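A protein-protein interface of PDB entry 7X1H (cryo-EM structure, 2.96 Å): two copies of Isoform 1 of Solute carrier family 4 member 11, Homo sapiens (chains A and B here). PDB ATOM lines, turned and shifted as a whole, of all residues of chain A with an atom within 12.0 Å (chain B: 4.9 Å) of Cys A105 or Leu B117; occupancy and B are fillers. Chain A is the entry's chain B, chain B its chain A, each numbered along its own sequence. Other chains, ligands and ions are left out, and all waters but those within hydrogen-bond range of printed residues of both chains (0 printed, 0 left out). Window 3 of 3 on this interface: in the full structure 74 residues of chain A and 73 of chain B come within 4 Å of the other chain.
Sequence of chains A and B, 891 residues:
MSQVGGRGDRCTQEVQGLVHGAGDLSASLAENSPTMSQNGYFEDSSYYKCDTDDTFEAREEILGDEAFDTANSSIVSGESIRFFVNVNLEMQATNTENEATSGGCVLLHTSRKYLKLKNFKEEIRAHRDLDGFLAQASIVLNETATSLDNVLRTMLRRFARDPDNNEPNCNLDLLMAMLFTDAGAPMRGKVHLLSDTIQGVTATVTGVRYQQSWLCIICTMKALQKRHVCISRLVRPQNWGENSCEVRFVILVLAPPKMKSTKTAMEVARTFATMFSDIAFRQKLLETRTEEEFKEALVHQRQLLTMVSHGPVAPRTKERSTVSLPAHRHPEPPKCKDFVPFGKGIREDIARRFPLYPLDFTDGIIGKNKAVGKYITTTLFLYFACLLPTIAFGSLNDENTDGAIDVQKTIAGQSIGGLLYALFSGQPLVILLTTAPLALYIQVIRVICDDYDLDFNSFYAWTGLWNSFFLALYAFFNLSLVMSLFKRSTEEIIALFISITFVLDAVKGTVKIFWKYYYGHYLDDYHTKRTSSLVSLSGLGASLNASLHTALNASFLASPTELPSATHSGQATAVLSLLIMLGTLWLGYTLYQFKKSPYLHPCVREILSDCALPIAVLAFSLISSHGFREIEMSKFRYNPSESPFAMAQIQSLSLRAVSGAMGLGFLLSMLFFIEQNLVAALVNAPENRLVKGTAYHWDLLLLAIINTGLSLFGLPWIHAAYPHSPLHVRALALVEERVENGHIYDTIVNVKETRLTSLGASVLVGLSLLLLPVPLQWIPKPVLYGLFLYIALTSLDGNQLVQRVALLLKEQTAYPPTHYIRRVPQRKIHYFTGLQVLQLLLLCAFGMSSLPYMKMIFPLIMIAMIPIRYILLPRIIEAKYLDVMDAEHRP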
ATOM      1  N   CYS A 105      22.174  -2.248  20.069  1.00  0.00           N
ATOM      2  CA  CYS A 105      23.126  -1.703  21.029  1.00  0.00           C
ATOM      3  C   CYS A 105      23.873  -2.822  21.744  1.00  0.00           C
ATOM      4  O   CYS A 105      23.446  -3.975  21.727  1.00  0.00           O
ATOM      5  CB  CYS A 105      22.413  -0.814  22.049  1.00  0.00           C
ATOM      6  SG  CYS A 105      21.620  -1.726  23.393  1.00  0.00           S
ATOM      7  N   VAL A 106      24.993  -2.471  22.373  1.00  0.00           N
ATOM      8  CA  VAL A 106      25.817  -3.414  23.116  1.00  0.00           C
ATOM      9  C   VAL A 106      26.029  -2.870  24.520  1.00  0.00           C
ATOM     10  O   VAL A 106      26.394  -1.702  24.695  1.00  0.00           O
ATOM     11  CB  VAL A 106      27.171  -3.662  22.418  1.00  0.00           C
ATOM     12  CG1 VAL A 106      26.954  -4.274  21.043  1.00  0.00           C
ATOM     13  CG2 VAL A 106      27.969  -2.370  22.312  1.00  0.00           C
ATOM     14  N   LEU A 107      25.795  -3.716  25.518  1.00  0.00           N
ATOM     15  CA  LEU A 107      25.998  -3.310  26.901  1.00  0.00           C
ATOM     16  C   LEU A 107      27.478  -3.068  27.167  1.00  0.00           C
ATOM     17  O   LEU A 107      28.343  -3.803  26.682  1.00  0.00           O
ATOM     18  CB  LEU A 107      25.463  -4.378  27.852  1.00  0.00           C
ATOM     19  CG  LEU A 107      23.971  -4.704  27.744  1.00  0.00           C
ATOM     20  CD1 LEU A 107      23.580  -5.734  28.790  1.00  0.00           C
ATOM     21  CD2 LEU A 107      23.126  -3.449  27.885  1.00  0.00           C
ATOM     22  N   LEU A 108      27.766  -2.027  27.943  1.00  0.00           N
ATOM     23  CA  LEU A 108      29.126  -1.660  28.306  1.00  0.00           C
ATOM     24  C   LEU A 108      29.265  -1.668  29.821  1.00  0.00           C
ATOM     25  O   LEU A 108      28.372  -1.206  30.536  1.00  0.00           O
ATOM     26  CB  LEU A 108      29.491  -0.279  27.754  1.00  0.00           C
ATOM     27  CG  LEU A 108      30.983  -0.022  27.532  1.00  0.00           C
ATOM     28  CD1 LEU A 108      31.470  -0.736  26.284  1.00  0.00           C
ATOM     29  CD2 LEU A 108      31.257   1.469  27.438  1.00  0.00           C
ATOM     30  N   HIS A 109      30.388  -2.194  30.304  1.00  0.00           N
ATOM     31  CA  HIS A 109      30.675  -2.280  31.733  1.00  0.00           C
ATOM     32  C   HIS A 109      31.856  -1.370  32.042  1.00  0.00           C
ATOM     33  O   HIS A 109      32.996  -1.681  31.682  1.00  0.00           O
ATOM     34  CB  HIS A 109      30.972  -3.721  32.144  1.00  0.00           C
ATOM     35  CG  HIS A 109      31.216  -3.891  33.613  1.00  0.00           C
ATOM     36  ND1 HIS A 109      32.193  -4.723  34.112  1.00  0.00           N
ATOM     37  CD2 HIS A 109      30.610  -3.334  34.687  1.00  0.00           C
ATOM     38  CE1 HIS A 109      32.179  -4.673  35.432  1.00  0.00           C
ATOM     39  NE2 HIS A 109      31.229  -3.836  35.806  1.00  0.00           N
ATOM     40  N   THR A 181      37.596  -2.040  23.190  1.00  0.00           N
ATOM     41  CA  THR A 181      36.563  -2.972  23.625  1.00  0.00           C
ATOM     42  C   THR A 181      36.143  -3.915  22.506  1.00  0.00           C
ATOM     43  O   THR A 181      35.691  -5.033  22.778  1.00  0.00           O
ATOM     44  CB  THR A 181      35.345  -2.205  24.140  1.00  0.00           C
ATOM     45  OG1 THR A 181      34.845  -1.346  23.109  1.00  0.00           O
ATOM     46  CG2 THR A 181      35.711  -1.372  25.358  1.00  0.00           C
ATOM     47  N   GLY A 189      31.630  -2.716  12.184  1.00  0.00           N
ATOM     48  CA  GLY A 189      31.563  -1.422  12.830  1.00  0.00           C
ATOM     49  C   GLY A 189      30.894  -1.481  14.187  1.00  0.00           C
ATOM     50  O   GLY A 189      29.680  -1.681  14.282  1.00  0.00           O
ATOM     51  N   LYS A 190      31.683  -1.310  15.247  1.00  0.00           N
ATOM     52  CA  LYS A 190      31.165  -1.341  16.608  1.00  0.00           C
ATOM     53  C   LYS A 190      31.685  -0.141  17.389  1.00  0.00           C
ATOM     54  O   LYS A 190      32.405   0.696  16.834  1.00  0.00           O
ATOM     55  CB  LYS A 190      31.561  -2.646  17.302  1.00  0.00           C
ATOM     56  CG  LYS A 190      30.692  -3.835  16.934  1.00  0.00           C
ATOM     57  CD  LYS A 190      31.161  -5.100  17.634  1.00  0.00           C
ATOM     58  CE  LYS A 190      30.295  -6.294  17.271  1.00  0.00           C
ATOM     59  NZ  LYS A 190      30.640  -7.498  18.076  1.00  0.00           N
ATOM     60  N   VAL A 191      31.333  -0.045  18.666  1.00  0.00           N
ATOM     61  CA  VAL A 191      31.837   1.033  19.509  1.00  0.00           C
ATOM     62  C   VAL A 191      33.333   0.834  19.706  1.00  0.00           C
ATOM     63  O   VAL A 191      33.785  -0.248  20.099  1.00  0.00           O
ATOM     64  CB  VAL A 191      31.092   1.075  20.853  1.00  0.00           C
ATOM     65  CG1 VAL A 191      29.623   1.396  20.633  1.00  0.00           C
ATOM     66  CG2 VAL A 191      31.241  -0.237  21.606  1.00  0.00           C
ATOM     67  N   HIS A 192      34.107   1.875  19.419  1.00  0.00           N
ATOM     68  CA  HIS A 192      35.566   1.812  19.405  1.00  0.00           C
ATOM     69  C   HIS A 192      36.072   2.631  20.593  1.00  0.00           C
ATOM     70  O   HIS A 192      36.363   3.821  20.467  1.00  0.00           O
ATOM     71  CB  HIS A 192      36.100   2.334  18.072  1.00  0.00           C
ATOM     72  CG  HIS A 192      37.572   2.137  17.884  1.00  0.00           C
ATOM     73  ND1 HIS A 192      38.126   0.909  17.597  1.00  0.00           N
ATOM     74  CD2 HIS A 192      38.601   3.016  17.916  1.00  0.00           C
ATOM     75  CE1 HIS A 192      39.435   1.036  17.473  1.00  0.00           C
ATOM     76  NE2 HIS A 192      39.748   2.305  17.659  1.00  0.00           N
ATOM     77  N   LEU A 193      36.174   1.978  21.749  1.00  0.00           N
ATOM     78  CA  LEU A 193      36.558   2.626  22.996  1.00  0.00           C
ATOM     79  C   LEU A 193      37.747   1.903  23.612  1.00  0.00           C
ATOM     80  O   LEU A 193      37.837   0.674  23.552  1.00  0.00           O
ATOM     81  CB  LEU A 193      35.393   2.638  23.991  1.00  0.00           C
ATOM     82  CG  LEU A 193      34.149   3.431  23.589  1.00  0.00           C
ATOM     83  CD1 LEU A 193      33.092   3.341  24.678  1.00  0.00           C
ATOM     84  CD2 LEU A 193      34.495   4.882  23.299  1.00  0.00           C
ATOM     85  N   LEU B 115      29.345  -6.624  27.282  1.00  0.00           N
ATOM     86  CA  LEU B 115      28.493  -7.592  27.957  1.00  0.00           C
ATOM     87  C   LEU B 115      27.409  -8.031  26.988  1.00  0.00           C
ATOM     88  O   LEU B 115      26.624  -7.204  26.514  1.00  0.00           O
ATOM     89  CB  LEU B 115      27.872  -7.003  29.228  1.00  0.00           C
ATOM     90  CG  LEU B 115      28.784  -6.959  30.455  1.00  0.00           C
ATOM     91  CD1 LEU B 115      28.136  -6.160  31.572  1.00  0.00           C
ATOM     92  CD2 LEU B 115      29.124  -8.363  30.933  1.00  0.00           C
ATOM     93  N   LYS B 116      27.370  -9.326  26.691  1.00  0.00           N
ATOM     94  CA  LYS B 116      26.399  -9.842  25.737  1.00  0.00           C
ATOM     95  C   LYS B 116      24.981  -9.657  26.265  1.00  0.00           C
ATOM     96  O   LYS B 116      24.695  -9.927  27.435  1.00  0.00           O
ATOM     97  CB  LYS B 116      26.661 -11.322  25.462  1.00  0.00           C
ATOM     98  CG  LYS B 116      27.966 -11.596  24.733  1.00  0.00           C
ATOM     99  CD  LYS B 116      28.087 -13.060  24.347  1.00  0.00           C
ATOM    100  CE  LYS B 116      28.383 -13.932  25.557  1.00  0.00           C
ATOM    101  NZ  LYS B 116      28.613 -15.355  25.183  1.00  0.00           N
ATOM    102  N   LEU B 117      24.091  -9.193  25.392  1.00  0.00           N
ATOM    103  CA  LEU B 117      22.690  -9.059  25.765  1.00  0.00           C
ATOM    104  C   LEU B 117      22.144 -10.410  26.208  1.00  0.00           C
ATOM    105  O   LEU B 117      22.388 -11.434  25.564  1.00  0.00           O
ATOM    106  CB  LEU B 117      21.880  -8.516  24.587  1.00  0.00           C
ATOM    107  CG  LEU B 117      22.072  -7.032  24.269  1.00  0.00           C
ATOM    108  CD1 LEU B 117      21.473  -6.695  22.914  1.00  0.00           C
ATOM    109  CD2 LEU B 117      21.458  -6.161  25.353  1.00  0.00           C
ATOM    110  N   LYS B 118      21.409 -10.410  27.317  1.00  0.00           N
ATOM    111  CA  LYS B 118      20.907 -11.658  27.875  1.00  0.00           C
ATOM    112  C   LYS B 118      20.040 -12.382  26.855  1.00  0.00           C
ATOM    113  O   LYS B 118      19.167 -11.780  26.222  1.00  0.00           O
ATOM    114  CB  LYS B 118      20.111 -11.379  29.151  1.00  0.00           C
ATOM    115  CG  LYS B 118      19.588 -12.627  29.853  1.00  0.00           C
ATOM    116  CD  LYS B 118      20.671 -13.294  30.684  1.00  0.00           C
ATOM    117  CE  LYS B 118      20.082 -14.273  31.685  1.00  0.00           C
ATOM    118  NZ  LYS B 118      19.114 -15.210  31.051  1.00  0.00           N
ATOM    119  N   ASN B 119      20.283 -13.681  26.700  1.00  0.00           N
ATOM    120  CA  ASN B 119      19.518 -14.529  25.788  1.00  0.00           C
ATOM    121  C   ASN B 119      18.456 -15.245  26.616  1.00  0.00           C
ATOM    122  O   ASN B 119      18.754 -16.206  27.331  1.00  0.00           O
ATOM    123  CB  ASN B 119      20.433 -15.513  25.066  1.00  0.00           C
ATOM    124  CG  ASN B 119      19.673 -16.457  24.151  1.00  0.00           C
ATOM    125  OD1 ASN B 119      18.447 -16.394  24.050  1.00  0.00           O
ATOM    126  ND2 ASN B 119      20.403 -17.339  23.479  1.00  0.00           N
ATOM    127  N   GLY B 200      23.630   1.483  28.034  1.00  0.00           N
ATOM    128  CA  GLY B 200      23.456   1.126  26.638  1.00  0.00           C
ATOM    129  C   GLY B 200      24.315   2.016  25.760  1.00  0.00           C
ATOM    130  O   GLY B 200      24.359   3.234  25.952  1.00  0.00           O
ATOM    131  N   VAL B 201      24.999   1.402  24.799  1.00  0.00           N
ATOM    132  CA  VAL B 201      25.940   2.104  23.934  1.00  0.00           C
ATOM    133  C   VAL B 201      25.722   1.656  22.497  1.00  0.00           C
ATOM    134  O   VAL B 201      25.461   0.476  22.237  1.00  0.00           O
ATOM    135  CB  VAL B 201      27.401   1.852  24.363  1.00  0.00           C
ATOM    136  CG1 VAL B 201      28.337   2.830  23.672  1.00  0.00           C
ATOM    137  CG2 VAL B 201      27.535   1.954  25.874  1.00  0.00           C
ATOM    138  N   THR B 202      25.827   2.600  21.564  1.00  0.00           N
ATOM    139  CA  THR B 202      25.707   2.317  20.143  1.00  0.00           C
ATOM    140  C   THR B 202      26.765   3.116  19.396  1.00  0.00           C
ATOM    141  O   THR B 202      27.267   4.129  19.886  1.00  0.00           O
ATOM    142  CB  THR B 202      24.306   2.662  19.615  1.00  0.00           C
ATOM    143  OG1 THR B 202      23.315   2.095  20.480  1.00  0.00           O
ATOM    144  CG2 THR B 202      24.110   2.122  18.205  1.00  0.00           C
ATOM    145  N   GLN B 211      23.176   5.394  25.870  1.00  0.00           N
ATOM    146  CA  GLN B 211      21.777   5.434  26.288  1.00  0.00           C
ATOM    147  C   GLN B 211      21.733   6.074  27.668  1.00  0.00           C
ATOM    148  O   GLN B 211      21.923   5.405  28.686  1.00  0.00           O
ATOM    149  CB  GLN B 211      21.172   4.037  26.293  1.00  0.00           C
ATOM    150  CG  GLN B 211      20.991   3.441  24.907  1.00  0.00           C
ATOM    151  CD  GLN B 211      19.984   2.309  24.881  1.00  0.00           C
ATOM    152  OE1 GLN B 211      19.120   2.212  25.752  1.00  0.00           O
ATOM    153  NE2 GLN B 211      20.089   1.446  23.879  1.00  0.00           N
ATOM    154  N   THR B 274      19.501  -5.743  29.661  1.00  0.00           N
ATOM    155  CA  THR B 274      18.905  -6.218  28.416  1.00  0.00           C
ATOM    156  C   THR B 274      17.430  -5.854  28.346  1.00  0.00           C
ATOM    157  O   THR B 274      16.943  -5.403  27.302  1.00  0.00           O
ATOM    158  CB  THR B 274      19.089  -7.730  28.290  1.00  0.00           C
ATOM    159  OG1 THR B 274      20.484  -8.051  28.340  1.00  0.00           O
ATOM    160  CG2 THR B 274      18.500  -8.238  26.983  1.00  0.00           C
ATOM    161  N   SER B 277      17.262  -2.018  27.926  1.00  0.00           N
ATOM    162  CA  SER B 277      17.848  -1.465  26.711  1.00  0.00           C
ATOM    163  C   SER B 277      16.815  -1.220  25.620  1.00  0.00           C
ATOM    164  O   SER B 277      17.111  -0.495  24.664  1.00  0.00           O
ATOM    165  CB  SER B 277      18.940  -2.397  26.185  1.00  0.00           C
ATOM    166  OG  SER B 277      18.385  -3.600  25.681  1.00  0.00           O
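Of chain B, only Leu B117 (3.6 Å), Val B201 (3.3 Å), Thr B202 (3.4 Å), Gln B211 (3.6 Å) and Ser B277 (3.9 Å) come within 4 Å of Cys A105.
Of the printed residues of chain B, His A109 touches Leu B115 (3.8 Å).
Gly A189 touches none of the printed residues of chain B.
Of the printed residues of chain B, Val A191 touches Val B201 and Thr B202.
His A192 touches none of the printed residues of chain B.
No residue of chain A comes within 4 Å of Lys B116.
Of chain A, only Cys A105 (3.6 Å) and Leu A107 (3.8 Å) come within 4 Å of Leu B117.
No residue of chain A comes within 4 Å of Asn B119.
Gly B200 touches none of the printed residues of chain A.
Val B201 touches just these residues of chain A: Cys A105 (3.3 Å), Val A106 (3.0 Å), Leu A108 (3.5 Å) and Val A191 (3.6 Å).
Of chain A, only Cys A105 (3.4 Å) and Val A191 (3.6 Å) come within 4 Å of Thr B202.
Of chain A, only Leu A107 comes within 4 Å of Thr B274.
Of the printed residues of chain A, Ser B277 touches Cys A105 (3.9 Å).
The nearest residue of chain A that does not touch Leu B117 is Val A106 (5.3 Å).
The nearest printed residue of chain B that does not touch Leu A107 is Lys B116 (4.5 Å).
Printed residues of chain B that touch a printed residue of chain A: Leu B115, Leu B117, Val B201, Thr B202, Gln B211, Thr B274 and Ser B277.
Hydrophobic or aromatic side chains of chain B within 4 Å of the printed part of chain A: Leu B115, Leu B117 and Val B201.
Of the 11 printed residues of chain A, 6 touch a printed residue of chain B.
Printed residues of chain A that touch a printed residue of chain B: Cys A105, Val A106, Leu A107, Leu A108, His A109 and Val A191.
Among the printed residues, no Asp or Glu carboxylate lies within 4 Å of a Lys or Arg side-chain nitrogen of the other chain.
CD1 of Leu B117 touches O of Cys A105, at 3.6 Å.
Cys A105 touches Val B201.
Thr B202 touches Cys A105 (OG1 to CB, 3.4 Å).
Cys A105 touches Ser B277.
Leu A107 touches Leu B117 (CG to CD2, 3.8 Å).
CD1 of Leu A107 touches OG1 of Thr B274 (3.9 Å).
CB of Leu A108 touches CG2 of Val B201, 3.5 Å away.
His A109 touches Leu B115.
Val B201 touches Val A191 (CG1 to CG1, 3.6 Å).
CG1 of Val A191 touches C of Thr B202, 3.6 Å away.
No position is printed for both chains.
Of the 13 pairs that touch across the chains among the printed residues, none has its exchanged pair printed and touching as well.
NE2 of Gln B211 is in hydrogen-bond range of SG of Cys A105.
The backbone NH (N) of Val A106 lies within hydrogen-bond range of the backbone carbonyl oxygen (O) of Val B201.
O of Leu A107 sits at hydrogen-bond distance from N of Leu B115, 3.1 Å away.
The backbone carbonyl oxygen (O) of Thr B274 lies within hydrogen-bond range of the side-chain hydroxyl (OG) of Ser B277 (2.8 Å).
The backbone NH (N) of Gln B211 is in hydrogen-bond range of the backbone carbonyl oxygen (O) of Gly B200 (2.5 Å).
OG1 of Thr A181 sits at hydrogen-bond distance from O of Val A191, 3.4 Å away.
The side-chain hydroxyl of Thr B274 sits at hydrogen-bond distance from the backbone NH of Lys B118 (2.7 Å).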
